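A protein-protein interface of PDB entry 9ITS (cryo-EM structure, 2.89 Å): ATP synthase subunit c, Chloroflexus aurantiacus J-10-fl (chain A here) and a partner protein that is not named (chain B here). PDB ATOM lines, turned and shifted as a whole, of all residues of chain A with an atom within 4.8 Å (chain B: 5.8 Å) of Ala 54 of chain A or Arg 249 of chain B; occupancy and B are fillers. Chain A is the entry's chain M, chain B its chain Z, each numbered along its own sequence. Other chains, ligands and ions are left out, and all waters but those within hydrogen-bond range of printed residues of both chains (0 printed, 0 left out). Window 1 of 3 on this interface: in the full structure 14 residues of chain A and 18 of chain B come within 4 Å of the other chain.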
ATOM      1  N   PHE A  50      17.296 -26.116 -10.593  1.00  0.00           N
ATOM      2  CA  PHE A  50      18.691 -25.960 -10.187  1.00  0.00           C
ATOM      3  C   PHE A  50      19.217 -27.191  -9.465  1.00  0.00           C
ATOM      4  O   PHE A  50      20.384 -27.551  -9.627  1.00  0.00           O
ATOM      5  CB  PHE A  50      18.882 -24.722  -9.306  1.00  0.00           C
ATOM      6  CG  PHE A  50      18.710 -23.414 -10.022  1.00  0.00           C
ATOM      7  CD1 PHE A  50      18.708 -23.351 -11.403  1.00  0.00           C
ATOM      8  CD2 PHE A  50      18.591 -22.236  -9.304  1.00  0.00           C
ATOM      9  CE1 PHE A  50      18.580 -22.136 -12.049  1.00  0.00           C
ATOM     10  CE2 PHE A  50      18.452 -21.023  -9.950  1.00  0.00           C
ATOM     11  CZ  PHE A  50      18.442 -20.976 -11.323  1.00  0.00           C
ATOM     12  N   ILE A  51      18.382 -27.839  -8.651  1.00  0.00           N
ATOM     13  CA  ILE A  51      18.819 -29.059  -7.968  1.00  0.00           C
ATOM     14  C   ILE A  51      19.187 -30.136  -8.986  1.00  0.00           C
ATOM     15  O   ILE A  51      20.242 -30.782  -8.890  1.00  0.00           O
ATOM     16  CB  ILE A  51      17.738 -29.552  -6.991  1.00  0.00           C
ATOM     17  CG1 ILE A  51      17.594 -28.583  -5.815  1.00  0.00           C
ATOM     18  CG2 ILE A  51      18.063 -30.949  -6.488  1.00  0.00           C
ATOM     19  CD1 ILE A  51      16.332 -28.787  -5.013  1.00  0.00           C
ATOM     20  N   GLY A  52      18.330 -30.330  -9.988  1.00  0.00           N
ATOM     21  CA  GLY A  52      18.623 -31.319 -11.014  1.00  0.00           C
ATOM     22  C   GLY A  52      19.847 -30.972 -11.841  1.00  0.00           C
ATOM     23  O   GLY A  52      20.673 -31.841 -12.146  1.00  0.00           O
ATOM     24  N   ILE A  53      19.973 -29.698 -12.227  1.00  0.00           N
ATOM     25  CA  ILE A  53      21.147 -29.259 -12.977  1.00  0.00           C
ATOM     26  C   ILE A  53      22.406 -29.457 -12.144  1.00  0.00           C
ATOM     27  O   ILE A  53      23.463 -29.834 -12.664  1.00  0.00           O
ATOM     28  CB  ILE A  53      20.978 -27.795 -13.423  1.00  0.00           C
ATOM     29  CG1 ILE A  53      19.819 -27.668 -14.410  1.00  0.00           C
ATOM     30  CG2 ILE A  53      22.253 -27.272 -14.059  1.00  0.00           C
ATOM     31  CD1 ILE A  53      20.110 -28.230 -15.775  1.00  0.00           C
ATOM     32  N   ALA A  54      22.305 -29.223 -10.835  1.00  0.00           N
ATOM     33  CA  ALA A  54      23.429 -29.435  -9.936  1.00  0.00           C
ATOM     34  C   ALA A  54      23.841 -30.897  -9.905  1.00  0.00           C
ATOM     35  O   ALA A  54      25.030 -31.212  -9.914  1.00  0.00           O
ATOM     36  CB  ALA A  54      23.067 -28.959  -8.534  1.00  0.00           C
ATOM     37  N   PHE A  55      22.866 -31.804  -9.851  1.00  0.00           N
ATOM     38  CA  PHE A  55      23.196 -33.229  -9.830  1.00  0.00           C
ATOM     39  C   PHE A  55      23.857 -33.664 -11.139  1.00  0.00           C
ATOM     40  O   PHE A  55      24.846 -34.416 -11.138  1.00  0.00           O
ATOM     41  CB  PHE A  55      21.934 -34.045  -9.554  1.00  0.00           C
ATOM     42  CG  PHE A  55      21.692 -34.314  -8.098  1.00  0.00           C
ATOM     43  CD1 PHE A  55      21.080 -33.364  -7.299  1.00  0.00           C
ATOM     44  CD2 PHE A  55      22.060 -35.522  -7.532  1.00  0.00           C
ATOM     45  CE1 PHE A  55      20.849 -33.608  -5.960  1.00  0.00           C
ATOM     46  CE2 PHE A  55      21.829 -35.773  -6.194  1.00  0.00           C
ATOM     47  CZ  PHE A  55      21.224 -34.815  -5.406  1.00  0.00           C
ATOM     48  N   THR A  56      23.324 -33.192 -12.271  1.00  0.00           N
ATOM     49  CA  THR A  56      23.923 -33.521 -13.565  1.00  0.00           C
ATOM     50  C   THR A  56      25.350 -32.987 -13.664  1.00  0.00           C
ATOM     51  O   THR A  56      26.274 -33.707 -14.072  1.00  0.00           O
ATOM     52  CB  THR A  56      23.069 -32.959 -14.701  1.00  0.00           C
ATOM     53  OG1 THR A  56      22.922 -31.545 -14.527  1.00  0.00           O
ATOM     54  CG2 THR A  56      21.697 -33.609 -14.721  1.00  0.00           C
ATOM     55  N   GLU A  57      25.548 -31.723 -13.283  1.00  0.00           N
ATOM     56  CA  GLU A  57      26.890 -31.156 -13.290  1.00  0.00           C
ATOM     57  C   GLU A  57      27.790 -31.852 -12.283  1.00  0.00           C
ATOM     58  O   GLU A  57      29.000 -31.911 -12.485  1.00  0.00           O
ATOM     59  CB  GLU A  57      26.842 -29.655 -13.007  1.00  0.00           C
ATOM     60  CG  GLU A  57      28.124 -28.929 -13.387  1.00  0.00           C
ATOM     61  CD  GLU A  57      27.965 -27.423 -13.413  1.00  0.00           C
ATOM     62  OE1 GLU A  57      27.529 -26.854 -12.391  1.00  0.00           O
ATOM     63  OE2 GLU A  57      28.283 -26.809 -14.453  1.00  0.00           O
ATOM     64  N   ALA A  58      27.222 -32.389 -11.202  1.00  0.00           N
ATOM     65  CA  ALA A  58      28.019 -33.152 -10.250  1.00  0.00           C
ATOM     66  C   ALA A  58      28.571 -34.412 -10.896  1.00  0.00           C
ATOM     67  O   ALA A  58      29.742 -34.750 -10.713  1.00  0.00           O
ATOM     68  CB  ALA A  58      27.180 -33.499  -9.020  1.00  0.00           C
ATOM     69  N   ILE A  61      31.248 -33.306 -13.401  1.00  0.00           N
ATOM     70  CA  ILE A  61      32.443 -32.856 -12.705  1.00  0.00           C
ATOM     71  C   ILE A  61      33.152 -34.025 -12.033  1.00  0.00           C
ATOM     72  O   ILE A  61      34.374 -34.007 -11.887  1.00  0.00           O
ATOM     73  CB  ILE A  61      32.068 -31.729 -11.718  1.00  0.00           C
ATOM     74  CG1 ILE A  61      31.781 -30.437 -12.487  1.00  0.00           C
ATOM     75  CG2 ILE A  61      33.164 -31.466 -10.720  1.00  0.00           C
ATOM     76  CD1 ILE A  61      32.939 -29.962 -13.337  1.00  0.00           C
ATOM     77  N   PHE B 244      31.189 -35.563  -0.430  1.00  0.00           N
ATOM     78  CA  PHE B 244      32.141 -35.736  -1.522  1.00  0.00           C
ATOM     79  C   PHE B 244      31.633 -35.067  -2.791  1.00  0.00           C
ATOM     80  O   PHE B 244      32.376 -34.346  -3.465  1.00  0.00           O
ATOM     81  CB  PHE B 244      32.402 -37.224  -1.760  1.00  0.00           C
ATOM     82  CG  PHE B 244      33.073 -37.913  -0.607  1.00  0.00           C
ATOM     83  CD1 PHE B 244      34.040 -37.260   0.139  1.00  0.00           C
ATOM     84  CD2 PHE B 244      32.735 -39.214  -0.268  1.00  0.00           C
ATOM     85  CE1 PHE B 244      34.661 -37.891   1.201  1.00  0.00           C
ATOM     86  CE2 PHE B 244      33.353 -39.850   0.794  1.00  0.00           C
ATOM     87  CZ  PHE B 244      34.317 -39.188   1.529  1.00  0.00           C
ATOM     88  N   ALA B 245      30.354 -35.273  -3.113  1.00  0.00           N
ATOM     89  CA  ALA B 245      29.767 -34.632  -4.284  1.00  0.00           C
ATOM     90  C   ALA B 245      29.761 -33.117  -4.142  1.00  0.00           C
ATOM     91  O   ALA B 245      30.105 -32.395  -5.086  1.00  0.00           O
ATOM     92  CB  ALA B 245      28.346 -35.150  -4.504  1.00  0.00           C
ATOM     93  N   LEU B 246      29.384 -32.618  -2.960  1.00  0.00           N
ATOM     94  CA  LEU B 246      29.280 -31.177  -2.755  1.00  0.00           C
ATOM     95  C   LEU B 246      30.637 -30.496  -2.893  1.00  0.00           C
ATOM     96  O   LEU B 246      30.742 -29.423  -3.498  1.00  0.00           O
ATOM     97  CB  LEU B 246      28.668 -30.886  -1.384  1.00  0.00           C
ATOM     98  CG  LEU B 246      27.165 -30.593  -1.333  1.00  0.00           C
ATOM     99  CD1 LEU B 246      26.353 -31.712  -1.968  1.00  0.00           C
ATOM    100  CD2 LEU B 246      26.711 -30.339   0.098  1.00  0.00           C
ATOM    101  N   ALA B 247      31.689 -31.105  -2.339  1.00  0.00           N
ATOM    102  CA  ALA B 247      33.020 -30.519  -2.454  1.00  0.00           C
ATOM    103  C   ALA B 247      33.565 -30.652  -3.870  1.00  0.00           C
ATOM    104  O   ALA B 247      34.134 -29.693  -4.418  1.00  0.00           O
ATOM    105  CB  ALA B 247      33.969 -31.178  -1.454  1.00  0.00           C
ATOM    106  N   PHE B 248      33.400 -31.833  -4.478  1.00  0.00           N
ATOM    107  CA  PHE B 248      33.951 -32.078  -5.801  1.00  0.00           C
ATOM    108  C   PHE B 248      33.303 -31.197  -6.856  1.00  0.00           C
ATOM    109  O   PHE B 248      33.988 -30.766  -7.785  1.00  0.00           O
ATOM    110  CB  PHE B 248      33.796 -33.553  -6.172  1.00  0.00           C
ATOM    111  CG  PHE B 248      34.839 -34.443  -5.561  1.00  0.00           C
ATOM    112  CD1 PHE B 248      36.074 -33.934  -5.197  1.00  0.00           C
ATOM    113  CD2 PHE B 248      34.585 -35.789  -5.352  1.00  0.00           C
ATOM    114  CE1 PHE B 248      37.038 -34.749  -4.635  1.00  0.00           C
ATOM    115  CE2 PHE B 248      35.545 -36.610  -4.790  1.00  0.00           C
ATOM    116  CZ  PHE B 248      36.773 -36.089  -4.432  1.00  0.00           C
ATOM    117  N   ARG B 249      32.004 -30.911  -6.727  1.00  0.00           N
ATOM    118  CA  ARG B 249      31.334 -30.049  -7.696  1.00  0.00           C
ATOM    119  C   ARG B 249      32.002 -28.682  -7.772  1.00  0.00           C
ATOM    120  O   ARG B 249      32.406 -28.234  -8.852  1.00  0.00           O
ATOM    121  CB  ARG B 249      29.860 -29.898  -7.323  1.00  0.00           C
ATOM    122  CG  ARG B 249      28.975 -29.381  -8.442  1.00  0.00           C
ATOM    123  CD  ARG B 249      27.737 -28.698  -7.880  1.00  0.00           C
ATOM    124  NE  ARG B 249      27.344 -29.247  -6.588  1.00  0.00           N
ATOM    125  CZ  ARG B 249      26.504 -30.260  -6.427  1.00  0.00           C
ATOM    126  NH1 ARG B 249      25.927 -30.850  -7.460  1.00  0.00           N
ATOM    127  NH2 ARG B 249      26.234 -30.689  -5.198  1.00  0.00           N
ATOM    128  N   LEU B 250      32.160 -28.022  -6.623  1.00  0.00           N
ATOM    129  CA  LEU B 250      32.779 -26.702  -6.600  1.00  0.00           C
ATOM    130  C   LEU B 250      34.238 -26.765  -7.035  1.00  0.00           C
ATOM    131  O   LEU B 250      34.689 -25.929  -7.833  1.00  0.00           O
ATOM    132  CB  LEU B 250      32.665 -26.093  -5.204  1.00  0.00           C
ATOM    133  CG  LEU B 250      31.333 -25.429  -4.852  1.00  0.00           C
ATOM    134  CD1 LEU B 250      31.391 -24.819  -3.461  1.00  0.00           C
ATOM    135  CD2 LEU B 250      30.971 -24.375  -5.885  1.00  0.00           C
ATOM    136  N   PHE B 251      34.987 -27.753  -6.530  1.00  0.00           N
ATOM    137  CA  PHE B 251      36.405 -27.846  -6.867  1.00  0.00           C
ATOM    138  C   PHE B 251      36.600 -28.034  -8.366  1.00  0.00           C
ATOM    139  O   PHE B 251      37.389 -27.319  -8.996  1.00  0.00           O
ATOM    140  CB  PHE B 251      37.053 -28.993  -6.089  1.00  0.00           C
ATOM    141  CG  PHE B 251      38.246 -29.596  -6.776  1.00  0.00           C
ATOM    142  CD1 PHE B 251      39.442 -28.901  -6.852  1.00  0.00           C
ATOM    143  CD2 PHE B 251      38.173 -30.857  -7.343  1.00  0.00           C
ATOM    144  CE1 PHE B 251      40.541 -29.451  -7.484  1.00  0.00           C
ATOM    145  CE2 PHE B 251      39.270 -31.413  -7.975  1.00  0.00           C
ATOM    146  CZ  PHE B 251      40.454 -30.708  -8.046  1.00  0.00           C
ATOM    147  N   GLY B 252      35.872 -28.983  -8.955  1.00  0.00           N
ATOM    148  CA  GLY B 252      36.003 -29.233 -10.377  1.00  0.00           C
ATOM    149  C   GLY B 252      35.516 -28.080 -11.226  1.00  0.00           C
ATOM    150  O   GLY B 252      36.124 -27.761 -12.248  1.00  0.00           O
ATOM    151  N   ASN B 253      34.421 -27.428 -10.817  1.00  0.00           N
ATOM    152  CA  ASN B 253      33.914 -26.296 -11.585  1.00  0.00           C
ATOM    153  C   ASN B 253      34.928 -25.160 -11.620  1.00  0.00           C
ATOM    154  O   ASN B 253      35.216 -24.604 -12.686  1.00  0.00           O
ATOM    155  CB  ASN B 253      32.587 -25.816 -10.998  1.00  0.00           C
ATOM    156  CG  ASN B 253      31.401 -26.591 -11.534  1.00  0.00           C
ATOM    157  OD1 ASN B 253      30.863 -26.270 -12.592  1.00  0.00           O
ATOM    158  ND2 ASN B 253      30.984 -27.616 -10.799  1.00  0.00           N
ATOM    159  N   ILE B 254      35.508 -24.826 -10.467  1.00  0.00           N
ATOM    160  CA  ILE B 254      36.457 -23.716 -10.430  1.00  0.00           C
ATOM    161  C   ILE B 254      37.762 -24.082 -11.132  1.00  0.00           C
ATOM    162  O   ILE B 254      38.349 -23.253 -11.842  1.00  0.00           O
ATOM    163  CB  ILE B 254      36.683 -23.265  -8.977  1.00  0.00           C
ATOM    164  CG1 ILE B 254      35.355 -22.802  -8.375  1.00  0.00           C
ATOM    165  CG2 ILE B 254      37.710 -22.146  -8.908  1.00  0.00           C
ATOM    166  CD1 ILE B 254      34.564 -21.870  -9.276  1.00  0.00           C
ATOM    167  N   GLN B 287      27.244 -21.096  -9.326  1.00  0.00           N
ATOM    168  CA  GLN B 287      27.703 -22.169  -8.453  1.00  0.00           C
ATOM    169  C   GLN B 287      27.532 -21.814  -6.985  1.00  0.00           C
ATOM    170  O   GLN B 287      27.242 -22.696  -6.169  1.00  0.00           O
ATOM    171  CB  GLN B 287      29.165 -22.501  -8.751  1.00  0.00           C
ATOM    172  CG  GLN B 287      29.356 -23.494  -9.885  1.00  0.00           C
ATOM    173  CD  GLN B 287      28.883 -24.889  -9.525  1.00  0.00           C
ATOM    174  OE1 GLN B 287      28.947 -25.300  -8.366  1.00  0.00           O
ATOM    175  NE2 GLN B 287      28.404 -25.627 -10.519  1.00  0.00           N
ATOM    176  N   ILE B 290      23.948 -22.397  -6.378  1.00  0.00           N
ATOM    177  CA  ILE B 290      23.740 -23.842  -6.396  1.00  0.00           C
ATOM    178  C   ILE B 290      24.136 -24.456  -5.063  1.00  0.00           C
ATOM    179  O   ILE B 290      23.394 -25.257  -4.490  1.00  0.00           O
ATOM    180  CB  ILE B 290      24.516 -24.488  -7.560  1.00  0.00           C
ATOM    181  CG1 ILE B 290      23.889 -24.132  -8.909  1.00  0.00           C
ATOM    182  CG2 ILE B 290      24.617 -25.986  -7.370  1.00  0.00           C
ATOM    183  CD1 ILE B 290      22.473 -24.610  -9.061  1.00  0.00           C
ATOM    184  N   PHE B 291      25.309 -24.090  -4.547  1.00  0.00           N
ATOM    185  CA  PHE B 291      25.753 -24.668  -3.286  1.00  0.00           C
ATOM    186  C   PHE B 291      24.798 -24.311  -2.154  1.00  0.00           C
ATOM    187  O   PHE B 291      24.397 -25.184  -1.372  1.00  0.00           O
ATOM    188  CB  PHE B 291      27.170 -24.205  -2.959  1.00  0.00           C
ATOM    189  CG  PHE B 291      27.873 -25.084  -1.972  1.00  0.00           C
ATOM    190  CD1 PHE B 291      27.706 -26.458  -2.012  1.00  0.00           C
ATOM    191  CD2 PHE B 291      28.688 -24.543  -0.995  1.00  0.00           C
ATOM    192  CE1 PHE B 291      28.348 -27.274  -1.104  1.00  0.00           C
ATOM    193  CE2 PHE B 291      29.328 -25.357  -0.085  1.00  0.00           C
ATOM    194  CZ  PHE B 291      29.159 -26.723  -0.139  1.00  0.00           C
ATOM    195  N   LEU B 294      21.324 -26.126  -2.730  1.00  0.00           N
ATOM    196  CA  LEU B 294      21.418 -27.568  -2.537  1.00  0.00           C
ATOM    197  C   LEU B 294      21.630 -27.933  -1.075  1.00  0.00           C
ATOM    198  O   LEU B 294      21.022 -28.892  -0.591  1.00  0.00           O
ATOM    199  CB  LEU B 294      22.519 -28.157  -3.420  1.00  0.00           C
ATOM    200  CG  LEU B 294      22.126 -28.554  -4.850  1.00  0.00           C
ATOM    201  CD1 LEU B 294      21.124 -29.691  -4.780  1.00  0.00           C
ATOM    202  CD2 LEU B 294      21.530 -27.417  -5.665  1.00  0.00           C
ATOM    203  N   PHE B 298      18.890 -30.056   0.921  1.00  0.00           N
ATOM    204  CA  PHE B 298      19.276 -31.292   1.589  1.00  0.00           C
ATOM    205  C   PHE B 298      18.867 -31.267   3.053  1.00  0.00           C
ATOM    206  O   PHE B 298      18.371 -32.268   3.583  1.00  0.00           O
ATOM    207  CB  PHE B 298      20.781 -31.521   1.446  1.00  0.00           C
ATOM    208  CG  PHE B 298      21.186 -32.045   0.098  1.00  0.00           C
ATOM    209  CD1 PHE B 298      20.375 -32.939  -0.581  1.00  0.00           C
ATOM    210  CD2 PHE B 298      22.373 -31.644  -0.491  1.00  0.00           C
ATOM    211  CE1 PHE B 298      20.740 -33.423  -1.823  1.00  0.00           C
ATOM    212  CE2 PHE B 298      22.745 -32.125  -1.732  1.00  0.00           C
ATOM    213  CZ  PHE B 298      21.927 -33.016  -2.398  1.00  0.00           C
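The guanidinium group of Arg 249 of chain B sits at hydrogen-bond distance from the backbone carbonyl oxygen of Ala 54 of chain A (2.6 Å).
The side-chain amide oxygen (OD1) of Asn 253 of chain B lies close to the side-chain carboxylate (OE2) of Glu 57 of chain A.
OE1 of Glu 57 of chain A is in hydrogen-bond range of NE2 of Gln 287 of chain B, 2.4 Å away.
The backbone carbonyl oxygen of Arg 249 of chain B is in hydrogen-bond range of the side-chain amide nitrogen of Asn 253 of chain B (2.5 Å).
The side-chain amide nitrogen (ND2) of Asn 253 of chain B lies close to the side-chain amide nitrogen (NE2) of Gln 287 of chain B (3.3 Å).
CB of Phe 50 of chain A touches CD1 of Ile 290 of chain B, at 3.6 Å.
Ala 54 of chain A touches Ile 290 of chain B (CB to CG2, 3.5 Å).
Leu 294 of chain B touches Ala 54 of chain A.
Phe 55 of chain A touches Arg 249 of chain B.
Phe 55 of chain A touches Phe 298 of chain B (CZ to CZ, 3.6 Å).
Arg 249 of chain B touches Ala 58 of chain A.
CG2 of Ile 61 of chain A touches O of Phe 248 of chain B, 3.1 Å away.
Ile 61 of chain A touches Arg 249 of chain B.
CA of Gly 252 of chain B touches CG2 of Ile 61 of chain A, 3.6 Å away.
Ile 61 of chain A touches Asn 253 of chain B (CG1 to ND2, 3.4 Å).
Of the printed residues of chain A, Arg 249 of chain B touches Ala 54, Phe 55, Ala 58 and Ile 61.
Printed residues of chain B within 4 Å of Glu 57 of chain A: Asn 253 and Gln 287.
Of the printed residues of chain B, Phe 55 of chain A touches Arg 249 and Phe 298.
Printed residues of chain A within 4 Å of Leu 294 of chain B: Ile 51 and Ala 54.
Of the printed residues of chain A, Gly 252 of chain B touches Ile 61.
The nearest printed residue of chain A that does not touch Phe 248 of chain B is Ala 58 of chain A (6.2 Å).
Along chain B the printed residues that touch a printed residue of chain A span positions 248 to 298.
Among the printed residues, 14 pairs touch across the chains.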
